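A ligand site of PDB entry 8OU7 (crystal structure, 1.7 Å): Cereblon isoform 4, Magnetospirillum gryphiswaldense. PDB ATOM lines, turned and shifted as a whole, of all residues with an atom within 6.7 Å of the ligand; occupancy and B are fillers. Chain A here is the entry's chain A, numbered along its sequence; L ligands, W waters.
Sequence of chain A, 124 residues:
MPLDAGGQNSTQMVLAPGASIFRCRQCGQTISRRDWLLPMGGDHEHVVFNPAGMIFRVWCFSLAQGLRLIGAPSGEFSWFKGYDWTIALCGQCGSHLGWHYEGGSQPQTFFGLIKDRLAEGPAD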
ATOM      1  N   VAL A  48      16.917   7.644 -34.478  1.00  0.00           N
ATOM      2  CA  VAL A  48      17.510   7.715 -33.166  1.00  0.00           C
ATOM      3  C   VAL A  48      18.972   7.353 -33.284  1.00  0.00           C
ATOM      4  O   VAL A  48      19.340   6.724 -34.262  1.00  0.00           O
ATOM      5  CB  VAL A  48      16.724   6.762 -32.224  1.00  0.00           C
ATOM      6  CG1 VAL A  48      15.283   7.213 -32.025  1.00  0.00           C
ATOM      7  CG2 VAL A  48      16.727   5.353 -32.759  1.00  0.00           C
ATOM      8  N   PHE A  49      19.789   7.701 -32.287  1.00  0.00           N
ATOM      9  CA  PHE A  49      21.137   7.201 -32.169  1.00  0.00           C
ATOM     10  C   PHE A  49      21.416   6.678 -30.775  1.00  0.00           C
ATOM     11  O   PHE A  49      20.837   7.104 -29.762  1.00  0.00           O
ATOM     12  CB  PHE A  49      22.137   8.266 -32.613  1.00  0.00           C
ATOM     13  CG  PHE A  49      22.205   9.468 -31.754  1.00  0.00           C
ATOM     14  CD1 PHE A  49      21.289  10.514 -31.856  1.00  0.00           C
ATOM     15  CD2 PHE A  49      23.256   9.589 -30.843  1.00  0.00           C
ATOM     16  CE1 PHE A  49      21.423  11.635 -31.051  1.00  0.00           C
ATOM     17  CE2 PHE A  49      23.411  10.739 -30.078  1.00  0.00           C
ATOM     18  CZ  PHE A  49      22.496  11.756 -30.168  1.00  0.00           C
ATOM     19  N   ASN A  50      22.323   5.738 -30.714  1.00  0.00           N
ATOM     20  CA  ASN A  50      22.702   5.106 -29.472  1.00  0.00           C
ATOM     21  C   ASN A  50      23.997   5.741 -28.926  1.00  0.00           C
ATOM     22  O   ASN A  50      24.547   6.666 -29.562  1.00  0.00           O
ATOM     23  CB  ASN A  50      22.742   3.589 -29.681  1.00  0.00           C
ATOM     24  CG  ASN A  50      23.906   3.093 -30.520  1.00  0.00           C
ATOM     25  OD1 ASN A  50      24.798   3.855 -30.874  1.00  0.00           O
ATOM     26  ND2 ASN A  50      23.962   1.788 -30.744  1.00  0.00           N
ATOM     27  N   PRO A  51      24.524   5.291 -27.781  1.00  0.00           N
ATOM     28  CA  PRO A  51      25.736   5.889 -27.217  1.00  0.00           C
ATOM     29  C   PRO A  51      26.981   5.631 -28.033  1.00  0.00           C
ATOM     30  O   PRO A  51      27.934   6.332 -27.829  1.00  0.00           O
ATOM     31  CB  PRO A  51      25.883   5.285 -25.818  1.00  0.00           C
ATOM     32  CG  PRO A  51      24.500   4.809 -25.485  1.00  0.00           C
ATOM     33  CD  PRO A  51      23.922   4.318 -26.806  1.00  0.00           C
ATOM     34  N   ALA A  52      26.945   4.680 -28.984  1.00  0.00           N
ATOM     35  CA  ALA A  52      28.033   4.411 -29.896  1.00  0.00           C
ATOM     36  C   ALA A  52      27.931   5.249 -31.170  1.00  0.00           C
ATOM     37  O   ALA A  52      28.725   5.001 -32.084  1.00  0.00           O
ATOM     38  CB  ALA A  52      28.166   2.961 -30.216  1.00  0.00           C
ATOM     39  N   MET A  54      25.658   5.153 -33.463  1.00  0.00           N
ATOM     40  CA  MET A  54      24.949   4.508 -34.547  1.00  0.00           C
ATOM     41  C   MET A  54      23.559   5.124 -34.668  1.00  0.00           C
ATOM     42  O   MET A  54      22.807   5.218 -33.691  1.00  0.00           O
ATOM     43  CB  MET A  54      24.845   3.007 -34.271  1.00  0.00           C
ATOM     44  CG  MET A  54      25.877   2.168 -34.940  1.00  0.00           C
ATOM     45  SD  MET A  54      25.202   0.543 -35.344  1.00  0.00           S
ATOM     46  CE  MET A  54      24.247   0.969 -36.803  1.00  0.00           C
ATOM     47  N   PHE A  56      19.786   4.817 -36.312  1.00  0.00           N
ATOM     48  CA  PHE A  56      18.821   3.796 -36.748  1.00  0.00           C
ATOM     49  C   PHE A  56      17.568   4.507 -37.162  1.00  0.00           C
ATOM     50  O   PHE A  56      17.072   5.433 -36.507  1.00  0.00           O
ATOM     51  CB  PHE A  56      18.517   2.855 -35.560  1.00  0.00           C
ATOM     52  CG  PHE A  56      19.660   2.055 -35.010  1.00  0.00           C
ATOM     53  CD1 PHE A  56      20.165   0.948 -35.649  1.00  0.00           C
ATOM     54  CD2 PHE A  56      20.347   2.539 -33.919  1.00  0.00           C
ATOM     55  CE1 PHE A  56      21.208   0.260 -35.082  1.00  0.00           C
ATOM     56  CE2 PHE A  56      21.368   1.822 -33.345  1.00  0.00           C
ATOM     57  CZ  PHE A  56      21.818   0.680 -33.920  1.00  0.00           C
ATOM     58  N   SER A  74      16.210  -3.429 -19.975  1.00  0.00           N
ATOM     59  CA  SER A  74      17.013  -2.336 -19.397  1.00  0.00           C
ATOM     60  C   SER A  74      16.348  -1.039 -19.790  1.00  0.00           C
ATOM     61  O   SER A  74      15.886  -0.860 -20.919  1.00  0.00           O
ATOM     62  CB  SER A  74      18.491  -2.413 -19.875  1.00  0.00           C
ATOM     63  OG  SER A  74      19.165  -1.197 -19.569  1.00  0.00           O
ATOM     64  N   GLU A  76      18.111   1.893 -19.620  1.00  0.00           N
ATOM     65  CA  GLU A  76      19.233   2.801 -19.889  1.00  0.00           C
ATOM     66  C   GLU A  76      19.188   3.302 -21.319  1.00  0.00           C
ATOM     67  O   GLU A  76      19.149   2.510 -22.257  1.00  0.00           O
ATOM     68  CB  GLU A  76      20.572   2.105 -19.641  1.00  0.00           C
ATOM     69  N   PHE A  77      19.144   4.617 -21.474  1.00  0.00           N
ATOM     70  CA  PHE A  77      19.167   5.259 -22.781  1.00  0.00           C
ATOM     71  C   PHE A  77      17.951   4.900 -23.646  1.00  0.00           C
ATOM     72  O   PHE A  77      17.978   5.075 -24.883  1.00  0.00           O
ATOM     73  CB  PHE A  77      20.467   4.957 -23.517  1.00  0.00           C
ATOM     74  CG  PHE A  77      21.752   5.283 -22.805  1.00  0.00           C
ATOM     75  CD1 PHE A  77      22.203   6.592 -22.720  1.00  0.00           C
ATOM     76  CD2 PHE A  77      22.581   4.283 -22.337  1.00  0.00           C
ATOM     77  CE1 PHE A  77      23.417   6.890 -22.121  1.00  0.00           C
ATOM     78  CE2 PHE A  77      23.769   4.573 -21.694  1.00  0.00           C
ATOM     79  CZ  PHE A  77      24.197   5.883 -21.614  1.00  0.00           C
ATOM     80  N   SER A  78      16.840   4.463 -23.050  1.00  0.00           N
ATOM     81  CA  SER A  78      15.658   4.187 -23.835  1.00  0.00           C
ATOM     82  C   SER A  78      15.189   5.403 -24.621  1.00  0.00           C
ATOM     83  O   SER A  78      14.983   6.453 -24.102  1.00  0.00           O
ATOM     84  CB  SER A  78      14.533   3.605 -23.005  1.00  0.00           C
ATOM     85  OG  SER A  78      13.415   3.319 -23.828  1.00  0.00           O
ATOM     86  N   TRP A  79      14.928   5.186 -25.913  1.00  0.00           N
ATOM     87  CA  TRP A  79      14.397   6.180 -26.802  1.00  0.00           C
ATOM     88  C   TRP A  79      12.921   6.468 -26.547  1.00  0.00           C
ATOM     89  O   TRP A  79      12.373   7.393 -27.133  1.00  0.00           O
ATOM     90  CB  TRP A  79      14.633   5.815 -28.278  1.00  0.00           C
ATOM     91  CG  TRP A  79      16.074   5.684 -28.633  1.00  0.00           C
ATOM     92  CD1 TRP A  79      17.078   6.567 -28.407  1.00  0.00           C
ATOM     93  CD2 TRP A  79      16.655   4.578 -29.328  1.00  0.00           C
ATOM     94  NE1 TRP A  79      18.274   6.067 -28.862  1.00  0.00           N
ATOM     95  CE2 TRP A  79      18.025   4.875 -29.504  1.00  0.00           C
ATOM     96  CE3 TRP A  79      16.173   3.347 -29.773  1.00  0.00           C
ATOM     97  CZ2 TRP A  79      18.916   3.990 -30.112  1.00  0.00           C
ATOM     98  CZ3 TRP A  79      17.059   2.504 -30.421  1.00  0.00           C
ATOM     99  CH2 TRP A  79      18.399   2.803 -30.588  1.00  0.00           C
ATOM    100  N   PHE A  80      12.203   5.582 -25.834  1.00  0.00           N
ATOM    101  CA  PHE A  80      10.781   5.686 -25.698  1.00  0.00           C
ATOM    102  C   PHE A  80      10.466   5.780 -24.209  1.00  0.00           C
ATOM    103  O   PHE A  80      10.854   4.947 -23.379  1.00  0.00           O
ATOM    104  CB  PHE A  80      10.064   4.489 -26.324  1.00  0.00           C
ATOM    105  CG  PHE A  80      10.298   4.378 -27.805  1.00  0.00           C
ATOM    106  CD1 PHE A  80       9.597   5.203 -28.675  1.00  0.00           C
ATOM    107  CD2 PHE A  80      11.276   3.568 -28.314  1.00  0.00           C
ATOM    108  CE1 PHE A  80       9.755   5.113 -30.030  1.00  0.00           C
ATOM    109  CE2 PHE A  80      11.463   3.506 -29.689  1.00  0.00           C
ATOM    110  CZ  PHE A  80      10.678   4.260 -30.538  1.00  0.00           C
ATOM    111  N   TYR A  83       9.622   3.024 -21.207  1.00  0.00           N
ATOM    112  CA  TYR A  83       9.824   1.646 -21.667  1.00  0.00           C
ATOM    113  C   TYR A  83      11.229   1.207 -21.422  1.00  0.00           C
ATOM    114  O   TYR A  83      12.193   1.986 -21.557  1.00  0.00           O
ATOM    115  CB  TYR A  83       9.486   1.472 -23.157  1.00  0.00           C
ATOM    116  CG  TYR A  83       8.079   1.777 -23.547  1.00  0.00           C
ATOM    117  CD1 TYR A  83       7.078   0.818 -23.483  1.00  0.00           C
ATOM    118  CD2 TYR A  83       7.702   3.058 -23.949  1.00  0.00           C
ATOM    119  CE1 TYR A  83       5.807   1.037 -23.922  1.00  0.00           C
ATOM    120  CE2 TYR A  83       6.372   3.331 -24.281  1.00  0.00           C
ATOM    121  CZ  TYR A  83       5.419   2.341 -24.196  1.00  0.00           C
ATOM    122  OH  TYR A  83       4.131   2.564 -24.564  1.00  0.00           O
ATOM    123  N   TRP A  85      13.996  -1.823 -22.670  1.00  0.00           N
ATOM    124  CA  TRP A  85      14.238  -2.546 -23.943  1.00  0.00           C
ATOM    125  C   TRP A  85      14.934  -3.858 -23.676  1.00  0.00           C
ATOM    126  O   TRP A  85      15.755  -3.970 -22.770  1.00  0.00           O
ATOM    127  CB  TRP A  85      15.025  -1.660 -24.924  1.00  0.00           C
ATOM    128  CG  TRP A  85      16.254  -1.040 -24.385  1.00  0.00           C
ATOM    129  CD1 TRP A  85      16.366   0.258 -23.882  1.00  0.00           C
ATOM    130  CD2 TRP A  85      17.538  -1.648 -24.248  1.00  0.00           C
ATOM    131  NE1 TRP A  85      17.619   0.414 -23.359  1.00  0.00           N
ATOM    132  CE2 TRP A  85      18.381  -0.683 -23.595  1.00  0.00           C
ATOM    133  CE3 TRP A  85      18.092  -2.875 -24.616  1.00  0.00           C
ATOM    134  CZ2 TRP A  85      19.692  -0.958 -23.313  1.00  0.00           C
ATOM    135  CZ3 TRP A  85      19.411  -3.134 -24.331  1.00  0.00           C
ATOM    136  CH2 TRP A  85      20.225  -2.156 -23.743  1.00  0.00           C
ATOM    137  N   ILE A  87      17.141  -6.510 -26.445  1.00  0.00           N
ATOM    138  CA  ILE A  87      17.647  -6.729 -27.815  1.00  0.00           C
ATOM    139  C   ILE A  87      16.838  -7.838 -28.474  1.00  0.00           C
ATOM    140  O   ILE A  87      16.563  -8.935 -27.868  1.00  0.00           O
ATOM    141  CB  ILE A  87      19.137  -7.078 -27.744  1.00  0.00           C
ATOM    142  CG1 ILE A  87      19.964  -5.867 -27.279  1.00  0.00           C
ATOM    143  CG2 ILE A  87      19.649  -7.536 -29.139  1.00  0.00           C
ATOM    144  CD1 ILE A  87      21.272  -6.241 -26.596  1.00  0.00           C
ATOM    145  N   HIS A  96      20.903  -8.705 -35.683  1.00  0.00           N
ATOM    146  CA  HIS A  96      20.196  -7.767 -34.802  1.00  0.00           C
ATOM    147  C   HIS A  96      19.117  -6.986 -35.565  1.00  0.00           C
ATOM    148  O   HIS A  96      19.435  -6.272 -36.529  1.00  0.00           O
ATOM    149  CB  HIS A  96      21.278  -6.794 -34.267  1.00  0.00           C
ATOM    150  CG  HIS A  96      20.605  -5.821 -33.388  1.00  0.00           C
ATOM    151  ND1 HIS A  96      21.005  -4.498 -33.339  1.00  0.00           N
ATOM    152  CD2 HIS A  96      19.528  -5.930 -32.524  1.00  0.00           C
ATOM    153  CE1 HIS A  96      20.284  -3.861 -32.407  1.00  0.00           C
ATOM    154  NE2 HIS A  96      19.379  -4.666 -31.920  1.00  0.00           N
ATOM    155  N   TRP A  99      14.629  -4.039 -31.166  1.00  0.00           N
ATOM    156  CA  TRP A  99      14.397  -4.158 -29.713  1.00  0.00           C
ATOM    157  C   TRP A  99      12.933  -4.418 -29.446  1.00  0.00           C
ATOM    158  O   TRP A  99      12.052  -3.947 -30.160  1.00  0.00           O
ATOM    159  CB  TRP A  99      14.860  -2.899 -28.937  1.00  0.00           C
ATOM    160  CG  TRP A  99      16.277  -2.500 -29.236  1.00  0.00           C
ATOM    161  CD1 TRP A  99      17.392  -2.831 -28.537  1.00  0.00           C
ATOM    162  CD2 TRP A  99      16.759  -1.771 -30.389  1.00  0.00           C
ATOM    163  NE1 TRP A  99      18.512  -2.359 -29.173  1.00  0.00           N
ATOM    164  CE2 TRP A  99      18.151  -1.692 -30.289  1.00  0.00           C
ATOM    165  CE3 TRP A  99      16.113  -1.146 -31.471  1.00  0.00           C
ATOM    166  CZ2 TRP A  99      18.930  -1.008 -31.228  1.00  0.00           C
ATOM    167  CZ3 TRP A  99      16.898  -0.522 -32.432  1.00  0.00           C
ATOM    168  CH2 TRP A  99      18.262  -0.441 -32.291  1.00  0.00           C
ATOM    169  N   TYR A 101      10.166  -3.526 -26.543  1.00  0.00           N
ATOM    170  CA  TYR A 101       9.950  -2.553 -25.461  1.00  0.00           C
ATOM    171  C   TYR A 101       8.805  -3.076 -24.561  1.00  0.00           C
ATOM    172  O   TYR A 101       7.809  -3.508 -25.032  1.00  0.00           O
ATOM    173  CB  TYR A 101       9.607  -1.211 -26.101  1.00  0.00           C
ATOM    174  CG  TYR A 101      10.793  -0.527 -26.710  1.00  0.00           C
ATOM    175  CD1 TYR A 101      11.699   0.168 -25.962  1.00  0.00           C
ATOM    176  CD2 TYR A 101      11.080  -0.738 -28.041  1.00  0.00           C
ATOM    177  CE1 TYR A 101      12.820   0.770 -26.541  1.00  0.00           C
ATOM    178  CE2 TYR A 101      12.226  -0.208 -28.630  1.00  0.00           C
ATOM    179  CZ  TYR A 101      13.102   0.538 -27.896  1.00  0.00           C
ATOM    180  OH  TYR A 101      14.245   1.081 -28.512  1.00  0.00           O
HETATM  181  C1  LIG L   1      20.001   1.321 -27.463  1.00  0.00           C
HETATM  182  N1  LIG L   1      21.295   0.978 -26.878  1.00  0.00           N
HETATM  183  C2  LIG L   1      17.612   0.687 -27.422  1.00  0.00           C
HETATM  184  C3  LIG L   1      17.220   2.029 -26.880  1.00  0.00           C
HETATM  185  C4  LIG L   1      19.564   2.704 -27.060  1.00  0.00           C
HETATM  186  C5  LIG L   1      22.316   0.578 -27.626  1.00  0.00           C
HETATM  187  C6  LIG L   1      26.311   0.615 -26.047  1.00  0.00           C
HETATM  188  C7  LIG L   1      26.008   0.310 -27.391  1.00  0.00           C
HETATM  189  C8  LIG L   1      24.716   0.296 -27.838  1.00  0.00           C
HETATM  190  C9  LIG L   1      23.007   0.992 -23.433  1.00  0.00           C
HETATM  191  C10 LIG L   1      18.997   0.262 -26.997  1.00  0.00           C
HETATM  192  N2  LIG L   1      18.230   2.966 -26.881  1.00  0.00           N
HETATM  193  O1  LIG L   1      20.414   3.562 -26.903  1.00  0.00           O
HETATM  194  O2  LIG L   1      16.086   2.379 -26.807  1.00  0.00           O
HETATM  195  O3  LIG L   1      22.165   0.435 -28.847  1.00  0.00           O
HETATM  196  C11 LIG L   1      23.650   0.569 -26.979  1.00  0.00           C
HETATM  197  C12 LIG L   1      23.955   0.877 -25.626  1.00  0.00           C
HETATM  198  C13 LIG L   1      25.269   0.933 -25.180  1.00  0.00           C
HETATM  199  N3  LIG L   1      27.640   0.609 -25.601  1.00  0.00           N
HETATM  200  O4  LIG L   1      22.921   1.264 -24.835  1.00  0.00           O
HETATM  201  O   HOH W   1      21.321  -2.449 -29.012  1.00  0.00           O
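Water W1 bridges NE1 of Trp 99 and O3 of the ligand.
The backbone carbonyl oxygen (O) of Tyr 83 lies within hydrogen-bond range of the side-chain hydroxyl (OG) of Ser 78 (2.9 Å). The indole nitrogen (NE1) of Trp 85 lies within hydrogen-bond range of the backbone carbonyl oxygen (O) of Glu 76 (2.8 Å). OD1 of Asn 50 is in hydrogen-bond range of N of Ala 52, at 3.0 Å. O of Ser 74 lies within hydrogen-bond range of N of Trp 85 (2.8 Å). OD1 of Asn 50 lies within hydrogen-bond range of N of Met 54 (3.0 Å). The backbone carbonyl oxygen (O) of Phe 49 sits at hydrogen-bond distance from the indole nitrogen (NE1) of Trp 79, at 2.9 Å. The side-chain hydroxyl (OG) of Ser 78 lies within hydrogen-bond range of the backbone carbonyl oxygen (O) of Phe 80, 3.1 Å away.
O of Phe 77 is in hydrogen-bond range of N2 of the ligand (2.9 Å). An oxygen (O2) of the ligand sits at hydrogen-bond distance from the side-chain hydroxyl (OH) of Tyr 101 (2.8 Å). The side-chain amide nitrogen (ND2) of Asn 50 is in hydrogen-bond range of an oxygen (O3) of the ligand. N of Trp 79 lies close to O2 of the ligand, 3.2 Å away.
Pro 51 touches the ligand (CD to O1, 3.6 Å). Ser 78 touches the ligand. Trp 85 touches the ligand. Trp 99 touches the ligand (NE1 to C10, 3.4 Å). Within 4 Å of the ligand: Asn 50, Pro 51, Phe 77, Ser 78, Trp 79, Trp 85, Trp 99 and Tyr 101.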
